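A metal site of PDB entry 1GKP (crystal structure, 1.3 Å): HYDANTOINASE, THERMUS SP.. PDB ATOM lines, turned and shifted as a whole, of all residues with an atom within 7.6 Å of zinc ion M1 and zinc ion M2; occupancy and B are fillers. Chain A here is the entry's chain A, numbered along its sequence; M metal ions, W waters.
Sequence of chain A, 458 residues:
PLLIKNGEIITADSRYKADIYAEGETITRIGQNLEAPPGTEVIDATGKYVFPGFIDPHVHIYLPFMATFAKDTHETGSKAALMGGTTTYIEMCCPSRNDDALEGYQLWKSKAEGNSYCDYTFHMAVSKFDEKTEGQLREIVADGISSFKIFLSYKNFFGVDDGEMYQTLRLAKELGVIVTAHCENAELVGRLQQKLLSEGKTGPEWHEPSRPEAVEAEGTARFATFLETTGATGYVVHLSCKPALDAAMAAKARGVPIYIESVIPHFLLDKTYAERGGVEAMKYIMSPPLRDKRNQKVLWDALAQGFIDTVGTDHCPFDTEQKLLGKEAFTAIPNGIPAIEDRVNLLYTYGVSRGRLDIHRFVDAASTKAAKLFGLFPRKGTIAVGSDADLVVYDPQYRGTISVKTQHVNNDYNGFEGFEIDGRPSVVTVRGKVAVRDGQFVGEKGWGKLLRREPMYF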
ATOM      1  N   HIS A  58      -0.234 -13.428  -5.882  1.00  0.00           N
ATOM      2  CA  HIS A  58       0.022 -13.989  -4.602  1.00  0.00           C
ATOM      3  C   HIS A  58       0.102 -15.522  -4.604  1.00  0.00           C
ATOM      4  O   HIS A  58      -0.941 -16.209  -4.526  1.00  0.00           O
ATOM      5  CB  HIS A  58      -1.068 -13.562  -3.606  1.00  0.00           C
ATOM      6  CG  HIS A  58      -0.765 -13.866  -2.176  1.00  0.00           C
ATOM      7  ND1 HIS A  58      -1.441 -13.272  -1.126  1.00  0.00           N
ATOM      8  CD2 HIS A  58       0.071 -14.750  -1.595  1.00  0.00           C
ATOM      9  CE1 HIS A  58      -1.003 -13.776   0.017  1.00  0.00           C
ATOM     10  NE2 HIS A  58      -0.093 -14.709  -0.214  1.00  0.00           N
ATOM     11  N   VAL A  59       1.311 -16.071  -4.754  1.00  0.00           N
ATOM     12  CA  VAL A  59       1.448 -17.528  -4.818  1.00  0.00           C
ATOM     13  C   VAL A  59       2.623 -17.948  -3.972  1.00  0.00           C
ATOM     14  O   VAL A  59       3.581 -17.152  -3.717  1.00  0.00           O
ATOM     15  CB  VAL A  59       1.519 -18.096  -6.300  1.00  0.00           C
ATOM     16  CG1 VAL A  59       0.362 -17.703  -7.156  1.00  0.00           C
ATOM     17  CG2 VAL A  59       2.891 -17.714  -6.917  1.00  0.00           C
ATOM     18  N   HIS A  60       2.706 -19.222  -3.667  1.00  0.00           N
ATOM     19  CA  HIS A  60       3.790 -19.821  -2.947  1.00  0.00           C
ATOM     20  C   HIS A  60       4.268 -21.037  -3.765  1.00  0.00           C
ATOM     21  O   HIS A  60       3.506 -21.941  -3.994  1.00  0.00           O
ATOM     22  CB  HIS A  60       3.403 -20.296  -1.561  1.00  0.00           C
ATOM     23  CG  HIS A  60       3.074 -19.163  -0.652  1.00  0.00           C
ATOM     24  ND1 HIS A  60       4.059 -18.443   0.013  1.00  0.00           N
ATOM     25  CD2 HIS A  60       1.892 -18.540  -0.368  1.00  0.00           C
ATOM     26  CE1 HIS A  60       3.451 -17.467   0.718  1.00  0.00           C
ATOM     27  NE2 HIS A  60       2.134 -17.502   0.525  1.00  0.00           N
ATOM     28  N   LEU A  63       8.424 -23.060  -0.712  1.00  0.00           N
ATOM     29  CA  LEU A  63       8.061 -22.710   0.668  1.00  0.00           C
ATOM     30  C   LEU A  63       8.349 -23.837   1.644  1.00  0.00           C
ATOM     31  O   LEU A  63       7.639 -24.856   1.676  1.00  0.00           O
ATOM     32  CB  LEU A  63       6.586 -22.305   0.762  1.00  0.00           C
ATOM     33  CG  LEU A  63       6.222 -21.733   2.132  1.00  0.00           C
ATOM     34  CD1 LEU A  63       6.892 -20.420   2.472  1.00  0.00           C
ATOM     35  CD2 LEU A  63       4.749 -21.592   2.253  1.00  0.00           C
ATOM     36  N   MET A  92       5.645 -14.986  -3.276  1.00  0.00           N
ATOM     37  CA  MET A  92       6.181 -14.534  -2.012  1.00  0.00           C
ATOM     38  C   MET A  92       7.506 -15.178  -1.709  1.00  0.00           C
ATOM     39  O   MET A  92       7.588 -16.387  -1.545  1.00  0.00           O
ATOM     40  CB  MET A  92       5.166 -14.840  -0.868  1.00  0.00           C
ATOM     41  CG  MET A  92       3.798 -14.194  -1.036  1.00  0.00           C
ATOM     42  SD  MET A  92       4.004 -12.420  -0.718  1.00  0.00           S
ATOM     43  CE  MET A  92       2.302 -11.905  -0.985  1.00  0.00           C
ATOM     44  N   CYS A  94      10.048 -15.827   0.873  1.00  0.00           N
ATOM     45  CA  CYS A  94       9.816 -15.911   2.330  1.00  0.00           C
ATOM     46  C   CYS A  94      10.935 -16.419   3.251  1.00  0.00           C
ATOM     47  O   CYS A  94      10.743 -17.332   4.024  1.00  0.00           O
ATOM     48  CB  CYS A  94       8.502 -16.679   2.640  1.00  0.00           C
ATOM     49  SG  CYS A  94       7.028 -16.044   1.905  1.00  0.00           S
ATOM     50  N   KCX A 149       6.983  -7.731   1.531  1.00  0.00           N
ATOM     51  CA  KCX A 149       5.938  -8.455   2.222  1.00  0.00           C
ATOM     52  CB  KCX A 149       5.876  -9.916   1.780  1.00  0.00           C
ATOM     53  CG  KCX A 149       4.960 -10.842   2.636  1.00  0.00           C
ATOM     54  CD  KCX A 149       3.458 -10.489   2.515  1.00  0.00           C
ATOM     55  CE  KCX A 149       2.584 -11.533   3.207  1.00  0.00           C
ATOM     56  NZ  KCX A 149       2.664 -12.775   2.467  1.00  0.00           N
ATOM     57  C   KCX A 149       6.281  -8.425   3.679  1.00  0.00           C
ATOM     58  O   KCX A 149       7.394  -8.736   4.094  1.00  0.00           O
ATOM     59  CX  KCX A 149       1.851 -13.792   2.729  1.00  0.00           C
ATOM     60  OQ1 KCX A 149       0.916 -13.701   3.632  1.00  0.00           O
ATOM     61  OQ2 KCX A 149       2.044 -14.883   2.074  1.00  0.00           O
ATOM     62  N   ILE A 150       5.316  -7.996   4.521  1.00  0.00           N
ATOM     63  CA  ILE A 150       5.453  -8.129   5.930  1.00  0.00           C
ATOM     64  C   ILE A 150       4.280  -8.988   6.527  1.00  0.00           C
ATOM     65  O   ILE A 150       3.258  -9.116   5.916  1.00  0.00           O
ATOM     66  CB  ILE A 150       5.568  -6.773   6.731  1.00  0.00           C
ATOM     67  CG1 ILE A 150       4.290  -5.946   6.622  1.00  0.00           C
ATOM     68  CG2 ILE A 150       6.807  -6.011   6.333  1.00  0.00           C
ATOM     69  CD1 ILE A 150       4.250  -4.709   7.537  1.00  0.00           C
ATOM     70  N   PHE A 151       4.589  -9.513   7.704  1.00  0.00           N
ATOM     71  CA  PHE A 151       3.635 -10.373   8.423  1.00  0.00           C
ATOM     72  C   PHE A 151       3.378  -9.805   9.787  1.00  0.00           C
ATOM     73  O   PHE A 151       4.284  -9.597  10.544  1.00  0.00           O
ATOM     74  CB  PHE A 151       4.220 -11.802   8.601  1.00  0.00           C
ATOM     75  CG  PHE A 151       4.419 -12.551   7.303  1.00  0.00           C
ATOM     76  CD1 PHE A 151       5.581 -12.382   6.566  1.00  0.00           C
ATOM     77  CD2 PHE A 151       3.450 -13.405   6.819  1.00  0.00           C
ATOM     78  CE1 PHE A 151       5.768 -13.119   5.415  1.00  0.00           C
ATOM     79  CE2 PHE A 151       3.608 -14.099   5.616  1.00  0.00           C
ATOM     80  CZ  PHE A 151       4.837 -13.974   4.948  1.00  0.00           C
ATOM     81  N   SER A 153       1.917 -11.523  12.201  1.00  0.00           N
ATOM     82  CA  SER A 153       1.573 -12.909  12.584  1.00  0.00           C
ATOM     83  C   SER A 153       2.838 -13.689  12.680  1.00  0.00           C
ATOM     84  O   SER A 153       3.921 -13.141  12.451  1.00  0.00           O
ATOM     85  CB  SER A 153       0.735 -13.516  11.537  1.00  0.00           C
ATOM     86  OG  SER A 153      -0.002 -14.532  12.210  1.00  0.00           O
ATOM     87  N   TYR A 154       2.750 -14.960  13.074  1.00  0.00           N
ATOM     88  CA  TYR A 154       3.858 -15.909  13.090  1.00  0.00           C
ATOM     89  C   TYR A 154       4.966 -15.400  13.974  1.00  0.00           C
ATOM     90  O   TYR A 154       6.080 -15.123  13.498  1.00  0.00           O
ATOM     91  CB  TYR A 154       4.295 -16.187  11.634  1.00  0.00           C
ATOM     92  CG  TYR A 154       3.205 -16.553  10.671  1.00  0.00           C
ATOM     93  CD1 TYR A 154       2.351 -17.663  10.906  1.00  0.00           C
ATOM     94  CD2 TYR A 154       2.986 -15.816   9.527  1.00  0.00           C
ATOM     95  CE1 TYR A 154       1.402 -17.992  10.058  1.00  0.00           C
ATOM     96  CE2 TYR A 154       2.028 -16.132   8.662  1.00  0.00           C
ATOM     97  CZ  TYR A 154       1.206 -17.231   8.910  1.00  0.00           C
ATOM     98  OH  TYR A 154       0.271 -17.459   7.965  1.00  0.00           O
ATOM     99  N   ALA A 181       1.073  -6.886   2.963  1.00  0.00           N
ATOM    100  CA  ALA A 181       1.076  -7.311   4.375  1.00  0.00           C
ATOM    101  C   ALA A 181      -0.042  -8.313   4.696  1.00  0.00           C
ATOM    102  O   ALA A 181      -1.183  -8.161   4.301  1.00  0.00           O
ATOM    103  CB  ALA A 181       0.804  -6.060   5.248  1.00  0.00           C
ATOM    104  N   HIS A 182       0.411  -9.366   5.392  1.00  0.00           N
ATOM    105  CA  HIS A 182      -0.457 -10.359   6.036  1.00  0.00           C
ATOM    106  C   HIS A 182      -0.837  -9.792   7.389  1.00  0.00           C
ATOM    107  O   HIS A 182      -0.022  -9.639   8.267  1.00  0.00           O
ATOM    108  CB  HIS A 182       0.301 -11.676   6.155  1.00  0.00           C
ATOM    109  CG  HIS A 182      -0.432 -12.726   6.935  1.00  0.00           C
ATOM    110  ND1 HIS A 182      -0.590 -14.007   6.457  1.00  0.00           N
ATOM    111  CD2 HIS A 182      -0.943 -12.715   8.196  1.00  0.00           C
ATOM    112  CE1 HIS A 182      -1.189 -14.723   7.405  1.00  0.00           C
ATOM    113  NE2 HIS A 182      -1.438 -13.955   8.467  1.00  0.00           N
ATOM    114  N   CYS A 183      -2.123  -9.471   7.536  1.00  0.00           N
ATOM    115  CA  CYS A 183      -2.598  -8.724   8.709  1.00  0.00           C
ATOM    116  C   CYS A 183      -3.422  -9.565   9.695  1.00  0.00           C
ATOM    117  O   CYS A 183      -4.616  -9.757   9.502  1.00  0.00           O
ATOM    118  CB  CYS A 183      -3.439  -7.564   8.231  1.00  0.00           C
ATOM    119  SG  CYS A 183      -2.461  -6.331   7.272  1.00  0.00           S
ATOM    120  N   GLU A 184      -2.722 -10.050  10.700  1.00  0.00           N
ATOM    121  CA  GLU A 184      -3.396 -10.722  11.851  1.00  0.00           C
ATOM    122  C   GLU A 184      -2.747 -10.054  13.080  1.00  0.00           C
ATOM    123  O   GLU A 184      -2.514  -8.814  13.077  1.00  0.00           O
ATOM    124  CB  GLU A 184      -3.300 -12.262  11.857  1.00  0.00           C
ATOM    125  CG  GLU A 184      -4.031 -12.914  10.732  1.00  0.00           C
ATOM    126  CD  GLU A 184      -3.896 -14.414  10.828  1.00  0.00           C
ATOM    127  OE1 GLU A 184      -2.733 -14.873  10.667  1.00  0.00           O
ATOM    128  OE2 GLU A 184      -4.913 -15.080  11.126  1.00  0.00           O
ATOM    129  N   VAL A 237      -2.862  -8.254   1.805  1.00  0.00           N
ATOM    130  CA  VAL A 237      -2.988  -9.554   1.112  1.00  0.00           C
ATOM    131  C   VAL A 237      -4.206 -10.335   1.734  1.00  0.00           C
ATOM    132  O   VAL A 237      -4.567 -10.121   2.879  1.00  0.00           O
ATOM    133  CB  VAL A 237      -1.709 -10.411   1.082  1.00  0.00           C
ATOM    134  CG1 VAL A 237      -0.570  -9.635   0.448  1.00  0.00           C
ATOM    135  CG2 VAL A 237      -1.345 -10.893   2.411  1.00  0.00           C
ATOM    136  N   HIS A 238      -4.775 -11.213   0.925  1.00  0.00           N
ATOM    137  CA  HIS A 238      -5.865 -12.140   1.359  1.00  0.00           C
ATOM    138  C   HIS A 238      -6.794 -11.589   2.465  1.00  0.00           C
ATOM    139  O   HIS A 238      -6.872 -12.164   3.540  1.00  0.00           O
ATOM    140  CB  HIS A 238      -5.339 -13.521   1.758  1.00  0.00           C
ATOM    141  CG  HIS A 238      -4.241 -13.558   2.737  1.00  0.00           C
ATOM    142  ND1 HIS A 238      -4.161 -12.710   3.849  1.00  0.00           N
ATOM    143  CD2 HIS A 238      -3.136 -14.347   2.773  1.00  0.00           C
ATOM    144  CE1 HIS A 238      -3.090 -13.062   4.550  1.00  0.00           C
ATOM    145  NE2 HIS A 238      -2.403 -14.033   3.902  1.00  0.00           N
ATOM    146  N   GLU A 261      -6.328  -6.899  -1.627  1.00  0.00           N
ATOM    147  CA  GLU A 261      -6.448  -8.191  -2.352  1.00  0.00           C
ATOM    148  C   GLU A 261      -7.327  -9.128  -1.555  1.00  0.00           C
ATOM    149  O   GLU A 261      -7.215  -9.167  -0.358  1.00  0.00           O
ATOM    150  CB  GLU A 261      -5.060  -8.821  -2.376  1.00  0.00           C
ATOM    151  CG  GLU A 261      -4.975 -10.213  -2.971  1.00  0.00           C
ATOM    152  CD  GLU A 261      -3.642 -10.818  -2.658  1.00  0.00           C
ATOM    153  OE1 GLU A 261      -3.444 -11.536  -1.648  1.00  0.00           O
ATOM    154  OE2 GLU A 261      -2.594 -10.548  -3.428  1.00  0.00           O
ATOM    155  N   VAL A 263      -8.409 -13.434  -1.946  1.00  0.00           N
ATOM    156  CA  VAL A 263      -8.020 -14.642  -2.674  1.00  0.00           C
ATOM    157  C   VAL A 263      -9.201 -15.586  -2.865  1.00  0.00           C
ATOM    158  O   VAL A 263     -10.142 -15.649  -2.031  1.00  0.00           O
ATOM    159  CB  VAL A 263      -6.817 -15.322  -2.011  1.00  0.00           C
ATOM    160  CG1 VAL A 263      -5.574 -14.396  -2.098  1.00  0.00           C
ATOM    161  CG2 VAL A 263      -7.058 -15.782  -0.627  1.00  0.00           C
ATOM    162  N   MET A 286      -6.145 -22.821   6.059  1.00  0.00           N
ATOM    163  CA  MET A 286      -5.205 -21.801   5.522  1.00  0.00           C
ATOM    164  C   MET A 286      -5.283 -20.657   6.520  1.00  0.00           C
ATOM    165  O   MET A 286      -6.123 -20.618   7.430  1.00  0.00           O
ATOM    166  CB  MET A 286      -5.640 -21.390   4.149  1.00  0.00           C
ATOM    167  CG  MET A 286      -7.006 -20.681   3.972  1.00  0.00           C
ATOM    168  SD  MET A 286      -7.269 -19.968   2.458  1.00  0.00           S
ATOM    169  CE  MET A 286      -6.050 -18.561   2.557  1.00  0.00           C
ATOM    170  N   SER A 287      -4.397 -19.696   6.354  1.00  0.00           N
ATOM    171  CA  SER A 287      -4.505 -18.455   7.149  1.00  0.00           C
ATOM    172  C   SER A 287      -4.382 -17.234   6.280  1.00  0.00           C
ATOM    173  O   SER A 287      -3.409 -17.150   5.513  1.00  0.00           O
ATOM    174  CB  SER A 287      -3.397 -18.380   8.160  1.00  0.00           C
ATOM    175  OG  SER A 287      -3.449 -19.437   9.116  1.00  0.00           O
ATOM    176  N   PRO A 288      -5.315 -16.292   6.399  1.00  0.00           N
ATOM    177  CA  PRO A 288      -6.414 -16.326   7.334  1.00  0.00           C
ATOM    178  C   PRO A 288      -7.360 -17.494   7.037  1.00  0.00           C
ATOM    179  O   PRO A 288      -7.541 -17.834   5.885  1.00  0.00           O
ATOM    180  CB  PRO A 288      -7.079 -14.954   7.138  1.00  0.00           C
ATOM    181  CG  PRO A 288      -6.191 -14.198   6.316  1.00  0.00           C
ATOM    182  CD  PRO A 288      -5.285 -15.072   5.599  1.00  0.00           C
ATOM    183  N   THR A 313      -4.569 -15.954  -5.319  1.00  0.00           N
ATOM    184  CA  THR A 313      -4.899 -17.293  -4.815  1.00  0.00           C
ATOM    185  C   THR A 313      -4.358 -17.612  -3.474  1.00  0.00           C
ATOM    186  O   THR A 313      -4.974 -18.352  -2.719  1.00  0.00           O
ATOM    187  CB  THR A 313      -4.420 -18.454  -5.785  1.00  0.00           C
ATOM    188  OG1 THR A 313      -3.012 -18.247  -5.962  1.00  0.00           O
ATOM    189  CG2 THR A 313      -5.210 -18.432  -7.109  1.00  0.00           C
ATOM    190  N   ASP A 314      -3.228 -17.033  -3.077  1.00  0.00           N
ATOM    191  CA  ASP A 314      -2.457 -17.521  -1.983  1.00  0.00           C
ATOM    192  C   ASP A 314      -2.196 -19.050  -2.181  1.00  0.00           C
ATOM    193  O   ASP A 314      -2.232 -19.869  -1.262  1.00  0.00           O
ATOM    194  CB  ASP A 314      -3.093 -17.312  -0.619  1.00  0.00           C
ATOM    195  CG  ASP A 314      -2.157 -17.549   0.503  1.00  0.00           C
ATOM    196  OD1 ASP A 314      -0.842 -17.511   0.351  1.00  0.00           O
ATOM    197  OD2 ASP A 314      -2.561 -17.637   1.694  1.00  0.00           O
ATOM    198  N   HIS A 315      -1.975 -19.406  -3.447  1.00  0.00           N
ATOM    199  CA  HIS A 315      -1.697 -20.802  -3.800  1.00  0.00           C
ATOM    200  C   HIS A 315      -0.696 -21.365  -2.913  1.00  0.00           C
ATOM    201  O   HIS A 315       0.479 -20.913  -2.854  1.00  0.00           O
ATOM    202  CB  HIS A 315      -1.234 -20.858  -5.276  1.00  0.00           C
ATOM    203  CG  HIS A 315      -0.844 -22.205  -5.750  1.00  0.00           C
ATOM    204  ND1 HIS A 315      -1.774 -23.169  -6.035  1.00  0.00           N
ATOM    205  CD2 HIS A 315       0.356 -22.728  -6.073  1.00  0.00           C
ATOM    206  CE1 HIS A 315      -1.161 -24.243  -6.491  1.00  0.00           C
ATOM    207  NE2 HIS A 315       0.132 -24.030  -6.456  1.00  0.00           N
ATOM    208  N   CYS A 316      -1.031 -22.513  -2.294  1.00  0.00           N
ATOM    209  CA  CYS A 316      -0.070 -22.990  -1.337  1.00  0.00           C
ATOM    210  C   CYS A 316      -0.374 -24.524  -1.181  1.00  0.00           C
ATOM    211  O   CYS A 316      -1.078 -24.889  -0.231  1.00  0.00           O
ATOM    212  CB  CYS A 316      -0.157 -22.289  -0.015  1.00  0.00           C
ATOM    213  SG  CYS A 316       1.326 -22.560   0.994  1.00  0.00           S
HETATM  214 ZN    ZN M   1      -0.402 -14.957   4.507  1.00  0.00          ZN
HETATM  215 ZN    ZN M   2       0.603 -16.188   1.273  1.00  0.00          ZN
HETATM  216  O   HOH W   1      -0.532 -16.279   2.919  1.00  0.00           O
HETATM  217  O   HOH W   2       0.713 -16.508   5.529  1.00  0.00           O
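A ring nitrogen (NE2) of His 182 sits at hydrogen-bond distance from the side-chain carboxylate (OE1) of Glu 184 (2.7 Å).
The side-chain carboxylate (OE1) of Glu 261 is in hydrogen-bond range of a ring nitrogen (ND1) of His 58.
N of His 238 is in hydrogen-bond range of OE1 of Glu 261, 2.9 Å away.
The backbone NH (N) of His 60 is in hydrogen-bond range of the backbone carbonyl oxygen (O) of His 315, 2.9 Å away.
SD of Met 92 lies within hydrogen-bond range of NZ of KCX 149 (3.5 Å).
The backbone NH of His 182 sits at hydrogen-bond distance from the backbone carbonyl oxygen of Ile 150 (2.9 Å).
O of His 58 is in hydrogen-bond range of OG1 of Thr 313 (3.2 Å).
Water W1 binds zinc ion M2, at 2.0 Å.
OQ2 of KCX 149 is bound to zinc ion M2 (2.1 Å).
NE2 of His 60 is bound to zinc ion M2.
OD1 of Asp 314 binds zinc ion M2.
NE2 of His 58 binds zinc ion M2 (2.2 Å).
Zinc ion M1 is bound by OQ1 of KCX 149 (2.0 Å), water W1 (2.1 Å), water W2 (2.2 Å), a ring nitrogen (ND1) of His 182 (2.2 Å) and a ring nitrogen (NE2) of His 238 (2.3 Å).
Residues that only touch zinc ion M1: Ser 287 (3.9 Å).
Of the 26 residues printed, 4 come within 4 Å of zinc ion M1.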
